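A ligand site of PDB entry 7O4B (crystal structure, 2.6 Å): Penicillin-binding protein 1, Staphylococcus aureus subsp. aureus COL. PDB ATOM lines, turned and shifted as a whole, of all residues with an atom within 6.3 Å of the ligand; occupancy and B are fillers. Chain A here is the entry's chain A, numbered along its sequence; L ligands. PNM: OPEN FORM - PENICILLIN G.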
ATOM      1  N   PRO A 249      -5.888  -4.543   1.776  1.00  0.00           N
ATOM      2  CA  PRO A 249      -6.154  -5.402   2.916  1.00  0.00           C
ATOM      3  C   PRO A 249      -5.428  -6.753   2.821  1.00  0.00           C
ATOM      4  O   PRO A 249      -5.013  -7.293   3.857  1.00  0.00           O
ATOM      5  CB  PRO A 249      -7.666  -5.612   2.893  1.00  0.00           C
ATOM      6  CG  PRO A 249      -8.108  -5.220   1.499  1.00  0.00           C
ATOM      7  CD  PRO A 249      -7.112  -4.170   1.045  1.00  0.00           C
ATOM      8  N   GLY A 250      -5.353  -7.286   1.600  1.00  0.00           N
ATOM      9  CA  GLY A 250      -4.931  -8.670   1.357  1.00  0.00           C
ATOM     10  C   GLY A 250      -6.082  -9.634   1.598  1.00  0.00           C
ATOM     11  O   GLY A 250      -7.236  -9.232   1.421  1.00  0.00           O
ATOM     12  N   SER A 251      -5.784 -10.870   1.998  1.00  0.00           N
ATOM     13  CA  SER A 251      -6.696 -12.029   1.820  1.00  0.00           C
ATOM     14  C   SER A 251      -7.792 -12.050   2.890  1.00  0.00           C
ATOM     15  O   SER A 251      -8.630 -12.981   2.866  1.00  0.00           O
ATOM     16  CB  SER A 251      -5.877 -13.309   1.760  1.00  0.00           C
ATOM     17  OG  SER A 251      -5.235 -13.412   0.453  1.00  0.00           O
ATOM     18  N   THR A 252      -7.818 -11.083   3.797  1.00  0.00           N
ATOM     19  CA  THR A 252      -8.914 -10.882   4.792  1.00  0.00           C
ATOM     20  C   THR A 252     -10.184 -10.524   4.018  1.00  0.00           C
ATOM     21  O   THR A 252     -11.294 -10.913   4.490  1.00  0.00           O
ATOM     22  CB  THR A 252      -8.540  -9.824   5.832  1.00  0.00           C
ATOM     23  OG1 THR A 252      -7.911  -8.674   5.249  1.00  0.00           O
ATOM     24  CG2 THR A 252      -7.624 -10.405   6.890  1.00  0.00           C
ATOM     25  N   LYS A 254     -11.171 -11.664   1.263  1.00  0.00           N
ATOM     26  CA  LYS A 254     -11.729 -12.816   0.530  1.00  0.00           C
ATOM     27  C   LYS A 254     -13.070 -13.214   1.145  1.00  0.00           C
ATOM     28  O   LYS A 254     -13.900 -13.781   0.436  1.00  0.00           O
ATOM     29  CB  LYS A 254     -10.780 -14.011   0.548  1.00  0.00           C
ATOM     30  CG  LYS A 254      -9.584 -13.872  -0.362  1.00  0.00           C
ATOM     31  CD  LYS A 254      -8.731 -15.121  -0.393  1.00  0.00           C
ATOM     32  CE  LYS A 254      -7.525 -14.990  -1.308  1.00  0.00           C
ATOM     33  NZ  LYS A 254      -6.524 -16.039  -1.035  1.00  0.00           N
ATOM     34  N   SER A 286      -0.891 -16.404  -9.772  1.00  0.00           N
ATOM     35  CA  SER A 286      -0.829 -17.812  -9.303  1.00  0.00           C
ATOM     36  C   SER A 286      -1.133 -17.905  -7.813  1.00  0.00           C
ATOM     37  O   SER A 286      -0.992 -16.895  -7.134  1.00  0.00           O
ATOM     38  CB  SER A 286       0.519 -18.411  -9.648  1.00  0.00           C
ATOM     39  OG  SER A 286       1.433 -17.368  -9.972  1.00  0.00           O
ATOM     40  N   ASP A 287      -1.494 -19.101  -7.345  1.00  0.00           N
ATOM     41  CA  ASP A 287      -1.593 -19.449  -5.901  1.00  0.00           C
ATOM     42  C   ASP A 287      -0.229 -19.177  -5.286  1.00  0.00           C
ATOM     43  O   ASP A 287       0.702 -18.871  -6.033  1.00  0.00           O
ATOM     44  CB  ASP A 287      -2.093 -20.876  -5.686  1.00  0.00           C
ATOM     45  CG  ASP A 287      -3.530 -21.044  -6.150  1.00  0.00           C
ATOM     46  OD1 ASP A 287      -4.212 -20.029  -6.325  1.00  0.00           O
ATOM     47  OD2 ASP A 287      -3.953 -22.176  -6.365  1.00  0.00           O
ATOM     48  N   TRP A 288      -0.153 -19.247  -3.957  1.00  0.00           N
ATOM     49  CA  TRP A 288       1.028 -18.722  -3.213  1.00  0.00           C
ATOM     50  C   TRP A 288       2.195 -19.695  -3.306  1.00  0.00           C
ATOM     51  O   TRP A 288       3.319 -19.201  -3.304  1.00  0.00           O
ATOM     52  CB  TRP A 288       0.659 -18.396  -1.775  1.00  0.00           C
ATOM     53  CG  TRP A 288       0.056 -19.520  -1.012  1.00  0.00           C
ATOM     54  CD1 TRP A 288      -1.265 -19.757  -0.837  1.00  0.00           C
ATOM     55  CD2 TRP A 288       0.746 -20.551  -0.301  1.00  0.00           C
ATOM     56  NE1 TRP A 288      -1.450 -20.857  -0.045  1.00  0.00           N
ATOM     57  CE2 TRP A 288      -0.238 -21.368   0.297  1.00  0.00           C
ATOM     58  CE3 TRP A 288       2.094 -20.845  -0.080  1.00  0.00           C
ATOM     59  CZ2 TRP A 288       0.082 -22.474   1.082  1.00  0.00           C
ATOM     60  CZ3 TRP A 288       2.412 -21.939   0.699  1.00  0.00           C
ATOM     61  CH2 TRP A 288       1.413 -22.750   1.258  1.00  0.00           C
ATOM     62  N   TYR A 304      -6.802 -22.963   2.360  1.00  0.00           N
ATOM     63  CA  TYR A 304      -5.429 -22.707   1.859  1.00  0.00           C
ATOM     64  C   TYR A 304      -5.227 -21.257   1.408  1.00  0.00           C
ATOM     65  O   TYR A 304      -4.088 -20.872   1.136  1.00  0.00           O
ATOM     66  CB  TYR A 304      -5.134 -23.547   0.611  1.00  0.00           C
ATOM     67  CG  TYR A 304      -4.897 -25.023   0.807  1.00  0.00           C
ATOM     68  CD1 TYR A 304      -4.478 -25.535   2.016  1.00  0.00           C
ATOM     69  CD2 TYR A 304      -5.080 -25.893  -0.255  1.00  0.00           C
ATOM     70  CE1 TYR A 304      -4.241 -26.889   2.173  1.00  0.00           C
ATOM     71  CE2 TYR A 304      -4.844 -27.253  -0.111  1.00  0.00           C
ATOM     72  CZ  TYR A 304      -4.425 -27.746   1.105  1.00  0.00           C
ATOM     73  OH  TYR A 304      -4.202 -29.075   1.307  1.00  0.00           O
ATOM     74  N   SER A 305      -6.283 -20.476   1.244  1.00  0.00           N
ATOM     75  CA  SER A 305      -6.169 -19.086   0.730  1.00  0.00           C
ATOM     76  C   SER A 305      -5.681 -19.160  -0.726  1.00  0.00           C
ATOM     77  O   SER A 305      -4.614 -18.610  -1.030  1.00  0.00           O
ATOM     78  CB  SER A 305      -5.263 -18.253   1.607  1.00  0.00           C
ATOM     79  OG  SER A 305      -5.413 -16.857   1.365  1.00  0.00           O
ATOM     80  N   SER A 306      -6.428 -19.830  -1.586  1.00  0.00           N
ATOM     81  CA  SER A 306      -6.091 -19.916  -3.033  1.00  0.00           C
ATOM     82  C   SER A 306      -6.573 -18.642  -3.714  1.00  0.00           C
ATOM     83  O   SER A 306      -7.770 -18.371  -3.664  1.00  0.00           O
ATOM     84  CB  SER A 306      -6.694 -21.135  -3.676  1.00  0.00           C
ATOM     85  OG  SER A 306      -6.875 -20.932  -5.066  1.00  0.00           O
ATOM     86  N   ASN A 307      -5.708 -17.905  -4.379  1.00  0.00           N
ATOM     87  CA  ASN A 307      -6.136 -16.749  -5.202  1.00  0.00           C
ATOM     88  C   ASN A 307      -6.921 -17.258  -6.417  1.00  0.00           C
ATOM     89  O   ASN A 307      -7.684 -16.480  -6.998  1.00  0.00           O
ATOM     90  CB  ASN A 307      -4.957 -15.885  -5.629  1.00  0.00           C
ATOM     91  CG  ASN A 307      -4.280 -15.166  -4.477  1.00  0.00           C
ATOM     92  OD1 ASN A 307      -4.439 -15.513  -3.306  1.00  0.00           O
ATOM     93  ND2 ASN A 307      -3.507 -14.161  -4.805  1.00  0.00           N
ATOM     94  N   PHE A 360      -8.503 -10.763  -3.975  1.00  0.00           N
ATOM     95  CA  PHE A 360      -7.681 -11.224  -2.834  1.00  0.00           C
ATOM     96  C   PHE A 360      -7.019 -10.015  -2.139  1.00  0.00           C
ATOM     97  O   PHE A 360      -6.053 -10.197  -1.389  1.00  0.00           O
ATOM     98  CB  PHE A 360      -6.682 -12.308  -3.269  1.00  0.00           C
ATOM     99  CG  PHE A 360      -5.852 -12.003  -4.500  1.00  0.00           C
ATOM    100  CD1 PHE A 360      -4.628 -11.347  -4.397  1.00  0.00           C
ATOM    101  CD2 PHE A 360      -6.272 -12.430  -5.752  1.00  0.00           C
ATOM    102  CE1 PHE A 360      -3.873 -11.092  -5.527  1.00  0.00           C
ATOM    103  CE2 PHE A 360      -5.516 -12.175  -6.882  1.00  0.00           C
ATOM    104  CZ  PHE A 360      -4.322 -11.501  -6.767  1.00  0.00           C
ATOM    105  N   GLY A 361      -7.545  -8.827  -2.380  1.00  0.00           N
ATOM    106  CA  GLY A 361      -7.331  -7.657  -1.509  1.00  0.00           C
ATOM    107  C   GLY A 361      -6.088  -6.915  -1.874  1.00  0.00           C
ATOM    108  O   GLY A 361      -5.395  -6.431  -0.947  1.00  0.00           O
ATOM    109  N   GLN A 362      -5.797  -6.792  -3.166  1.00  0.00           N
ATOM    110  CA  GLN A 362      -4.796  -5.828  -3.676  1.00  0.00           C
ATOM    111  C   GLN A 362      -5.535  -4.862  -4.600  1.00  0.00           C
ATOM    112  O   GLN A 362      -6.688  -5.149  -4.885  1.00  0.00           O
ATOM    113  CB  GLN A 362      -3.664  -6.589  -4.365  1.00  0.00           C
ATOM    114  CG  GLN A 362      -3.092  -7.704  -3.516  1.00  0.00           C
ATOM    115  CD  GLN A 362      -1.896  -7.256  -2.685  1.00  0.00           C
ATOM    116  OE1 GLN A 362      -1.508  -6.072  -2.629  1.00  0.00           O
ATOM    117  NE2 GLN A 362      -1.271  -8.240  -2.065  1.00  0.00           N
ATOM    118  N   LYS A 450      -9.727 -15.160   9.380  1.00  0.00           N
ATOM    119  CA  LYS A 450      -9.090 -15.230   8.043  1.00  0.00           C
ATOM    120  C   LYS A 450      -7.800 -14.413   8.091  1.00  0.00           C
ATOM    121  O   LYS A 450      -7.853 -13.282   8.577  1.00  0.00           O
ATOM    122  CB  LYS A 450     -10.055 -14.701   6.983  1.00  0.00           C
ATOM    123  CG  LYS A 450      -9.483 -14.677   5.575  1.00  0.00           C
ATOM    124  CD  LYS A 450      -9.507 -16.040   4.912  1.00  0.00           C
ATOM    125  CE  LYS A 450      -8.689 -16.108   3.645  1.00  0.00           C
ATOM    126  NZ  LYS A 450      -7.234 -16.118   3.906  1.00  0.00           N
ATOM    127  N   THR A 451      -6.694 -15.000   7.616  1.00  0.00           N
ATOM    128  CA  THR A 451      -5.336 -14.421   7.581  1.00  0.00           C
ATOM    129  C   THR A 451      -5.167 -13.582   6.330  1.00  0.00           C
ATOM    130  O   THR A 451      -5.976 -13.708   5.400  1.00  0.00           O
ATOM    131  CB  THR A 451      -4.278 -15.540   7.535  1.00  0.00           C
ATOM    132  OG1 THR A 451      -4.528 -16.173   6.283  1.00  0.00           O
ATOM    133  CG2 THR A 451      -4.374 -16.505   8.692  1.00  0.00           C
ATOM    134  N   GLY A 452      -4.132 -12.759   6.291  1.00  0.00           N
ATOM    135  CA  GLY A 452      -3.841 -11.920   5.118  1.00  0.00           C
ATOM    136  C   GLY A 452      -2.363 -11.596   5.072  1.00  0.00           C
ATOM    137  O   GLY A 452      -1.828 -11.244   6.124  1.00  0.00           O
ATOM    138  N   THR A 453      -1.737 -11.777   3.911  1.00  0.00           N
ATOM    139  CA  THR A 453      -0.362 -11.301   3.615  1.00  0.00           C
ATOM    140  C   THR A 453      -0.424 -10.566   2.284  1.00  0.00           C
ATOM    141  O   THR A 453      -0.905 -11.159   1.324  1.00  0.00           O
ATOM    142  CB  THR A 453       0.640 -12.451   3.598  1.00  0.00           C
ATOM    143  OG1 THR A 453       0.489 -13.251   4.775  1.00  0.00           O
ATOM    144  CG2 THR A 453       2.057 -11.950   3.458  1.00  0.00           C
ATOM    145  N   ALA A 454       0.006  -9.298   2.235  1.00  0.00           N
ATOM    146  CA  ALA A 454      -0.313  -8.368   1.132  1.00  0.00           C
ATOM    147  C   ALA A 454       0.873  -7.488   0.830  1.00  0.00           C
ATOM    148  O   ALA A 454       1.609  -7.147   1.736  1.00  0.00           O
ATOM    149  CB  ALA A 454      -1.498  -7.508   1.488  1.00  0.00           C
ATOM    150  N   GLN A 455       1.017  -7.105  -0.434  1.00  0.00           N
ATOM    151  CA  GLN A 455       2.103  -6.215  -0.868  1.00  0.00           C
ATOM    152  C   GLN A 455       1.647  -4.804  -0.500  1.00  0.00           C
ATOM    153  O   GLN A 455       0.425  -4.534  -0.555  1.00  0.00           O
ATOM    154  CB  GLN A 455       2.399  -6.395  -2.345  1.00  0.00           C
ATOM    155  CG  GLN A 455       3.005  -7.758  -2.707  1.00  0.00           C
ATOM    156  CD  GLN A 455       3.481  -7.700  -4.141  1.00  0.00           C
ATOM    157  OE1 GLN A 455       2.714  -7.898  -5.084  1.00  0.00           O
ATOM    158  NE2 GLN A 455       4.724  -7.320  -4.323  1.00  0.00           N
ATOM    159  N   TYR A 471       5.643  -7.097   3.397  1.00  0.00           N
ATOM    160  CA  TYR A 471       4.203  -7.428   3.488  1.00  0.00           C
ATOM    161  C   TYR A 471       3.521  -6.659   4.629  1.00  0.00           C
ATOM    162  O   TYR A 471       4.172  -6.232   5.594  1.00  0.00           O
ATOM    163  CB  TYR A 471       4.006  -8.937   3.677  1.00  0.00           C
ATOM    164  CG  TYR A 471       4.679  -9.755   2.605  1.00  0.00           C
ATOM    165  CD1 TYR A 471       4.572  -9.386   1.279  1.00  0.00           C
ATOM    166  CD2 TYR A 471       5.445 -10.876   2.909  1.00  0.00           C
ATOM    167  CE1 TYR A 471       5.200 -10.088   0.271  1.00  0.00           C
ATOM    168  CE2 TYR A 471       6.085 -11.595   1.915  1.00  0.00           C
ATOM    169  CZ  TYR A 471       5.957 -11.204   0.590  1.00  0.00           C
ATOM    170  OH  TYR A 471       6.540 -11.865  -0.439  1.00  0.00           O
ATOM    171  N   SER A 474      -1.834  -9.534   8.536  1.00  0.00           N
ATOM    172  CA  SER A 474      -3.108  -9.155   9.195  1.00  0.00           C
ATOM    173  C   SER A 474      -3.924 -10.401   9.510  1.00  0.00           C
ATOM    174  O   SER A 474      -3.648 -11.445   8.979  1.00  0.00           O
ATOM    175  CB  SER A 474      -3.875  -8.180   8.355  1.00  0.00           C
ATOM    176  OG  SER A 474      -4.455  -8.772   7.205  1.00  0.00           O
ATOM    177  N   TYR A 503       6.075 -12.831   8.080  1.00  0.00           N
ATOM    178  CA  TYR A 503       5.437 -13.602   6.978  1.00  0.00           C
ATOM    179  C   TYR A 503       4.840 -14.911   7.527  1.00  0.00           C
ATOM    180  O   TYR A 503       3.690 -15.220   7.189  1.00  0.00           O
ATOM    181  CB  TYR A 503       6.420 -13.846   5.822  1.00  0.00           C
ATOM    182  CG  TYR A 503       5.882 -14.798   4.795  1.00  0.00           C
ATOM    183  CD1 TYR A 503       4.812 -14.418   4.009  1.00  0.00           C
ATOM    184  CD2 TYR A 503       6.356 -16.085   4.658  1.00  0.00           C
ATOM    185  CE1 TYR A 503       4.229 -15.303   3.114  1.00  0.00           C
ATOM    186  CE2 TYR A 503       5.804 -16.978   3.754  1.00  0.00           C
ATOM    187  CZ  TYR A 503       4.724 -16.580   2.977  1.00  0.00           C
ATOM    188  OH  TYR A 503       4.108 -17.408   2.077  1.00  0.00           O
HETATM  189  O8  PNM L   1      -3.640 -11.808   0.642  1.00  0.00           O
HETATM  190  C7  PNM L   1      -4.004 -12.909   0.289  1.00  0.00           C
HETATM  191  N4  PNM L   1      -2.892 -14.700   1.882  1.00  0.00           N
HETATM  192  C3  PNM L   1      -1.709 -15.184   2.653  1.00  0.00           C
HETATM  193  C11 PNM L   1      -2.286 -15.785   3.944  1.00  0.00           C
HETATM  194  O13 PNM L   1      -1.615 -15.552   4.992  1.00  0.00           O
HETATM  195  O12 PNM L   1      -3.384 -16.438   3.799  1.00  0.00           O
HETATM  196  C2  PNM L   1      -0.871 -16.244   1.807  1.00  0.00           C
HETATM  197  C10 PNM L   1      -1.073 -17.700   2.190  1.00  0.00           C
HETATM  198  C9  PNM L   1       0.610 -15.881   1.797  1.00  0.00           C
HETATM  199  S1  PNM L   1      -1.450 -16.031   0.050  1.00  0.00           S
HETATM  200  C5  PNM L   1      -2.999 -15.151   0.483  1.00  0.00           C
HETATM  201  C6  PNM L   1      -3.059 -13.897  -0.361  1.00  0.00           C
HETATM  202  N14 PNM L   1      -1.736 -13.292  -0.489  1.00  0.00           N
HETATM  203  C15 PNM L   1      -1.096 -13.301  -1.650  1.00  0.00           C
HETATM  204  O16 PNM L   1      -1.444 -14.055  -2.564  1.00  0.00           O
HETATM  205  C17 PNM L   1       0.139 -12.424  -1.754  1.00  0.00           C
HETATM  206  C18 PNM L   1       1.333 -13.173  -1.188  1.00  0.00           C
HETATM  207  C19 PNM L   1       2.089 -12.631  -0.162  1.00  0.00           C
HETATM  208  C20 PNM L   1       3.185 -13.311   0.371  1.00  0.00           C
HETATM  209  C21 PNM L   1       3.555 -14.553  -0.123  1.00  0.00           C
HETATM  210  C22 PNM L   1       2.810 -15.107  -1.144  1.00  0.00           C
HETATM  211  C23 PNM L   1       1.706 -14.431  -1.667  1.00  0.00           C
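The side-chain hydroxyl (OG1) of Thr 451 is in hydrogen-bond range of an oxygen (O12) of the ligand (2.7 Å). O12 of the ligand lies within salt-bridge range of NZ of Lys 450, 3.9 Å away. OG1 of Thr 453 sits at hydrogen-bond distance from O13 of the ligand (3.1 Å). The backbone NH (N) of Ser 251 is in hydrogen-bond range of an oxygen (O8) of the ligand, at 2.7 Å. O of Thr 453 sits at hydrogen-bond distance from N14 of the ligand (2.9 Å). The side-chain hydroxyl (OG) of Ser 251 is bonded to a carbon (C7) of the ligand, at 1.3 Å. O16 of the ligand lies within hydrogen-bond range of ND2 of Asn 307 (3.0 Å). The side-chain hydroxyl (OG) of Ser 305 sits close to an oxygen (O12) of the ligand.
The side-chain amino group of Lys 254 lies within hydrogen-bond range of the side-chain hydroxyl of Ser 251, at 3.3 Å. The backbone NH (N) of Ser 474 sits at hydrogen-bond distance from the backbone carbonyl oxygen (O) of Gly 452 (3.0 Å). N of Gly 250 is in hydrogen-bond range of O of Gly 361 (2.7 Å). N of Asn 307 sits at hydrogen-bond distance from OD1 of Asp 287. NE1 of Trp 288 lies within hydrogen-bond range of O of Tyr 304, at 2.9 Å. The side-chain hydroxyl of Ser 305 sits at hydrogen-bond distance from the side-chain amino group of Lys 254 (2.8 Å). The backbone NH (N) of Ser 251 sits at hydrogen-bond distance from the backbone carbonyl oxygen (O) of Phe 360 (3.5 Å). The side-chain hydroxyl of Ser 305 is in hydrogen-bond range of the side-chain amino group of Lys 450, 3.2 Å away.
Gly 250 touches the ligand. NZ of Lys 254 touches C5 of the ligand, 3.9 Å away. Trp 288 touches the ligand. Phe 360 touches the ligand (O to O8, 3.5 Å). Gly 452 touches the ligand (N to O13, 3.98 Å). Tyr 471 touches the ligand (CZ to C20, 3.5 Å). Tyr 503 touches the ligand (CE1 to C21, 3.4 Å). Hydrophobic or aromatic side chains within 4 Å of the ligand: Trp 288, Tyr 471 and Tyr 503. 13 residues have an atom within 4 Å of the ligand: Gly 250, Ser 251, Lys 254, Trp 288, Ser 305, Asn 307, Phe 360, Lys 450, Thr 451, Gly 452, Thr 453, Tyr 471 and Tyr 503. The nearest printed residue that does not touch the ligand is Gln 362 (4.4 Å).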
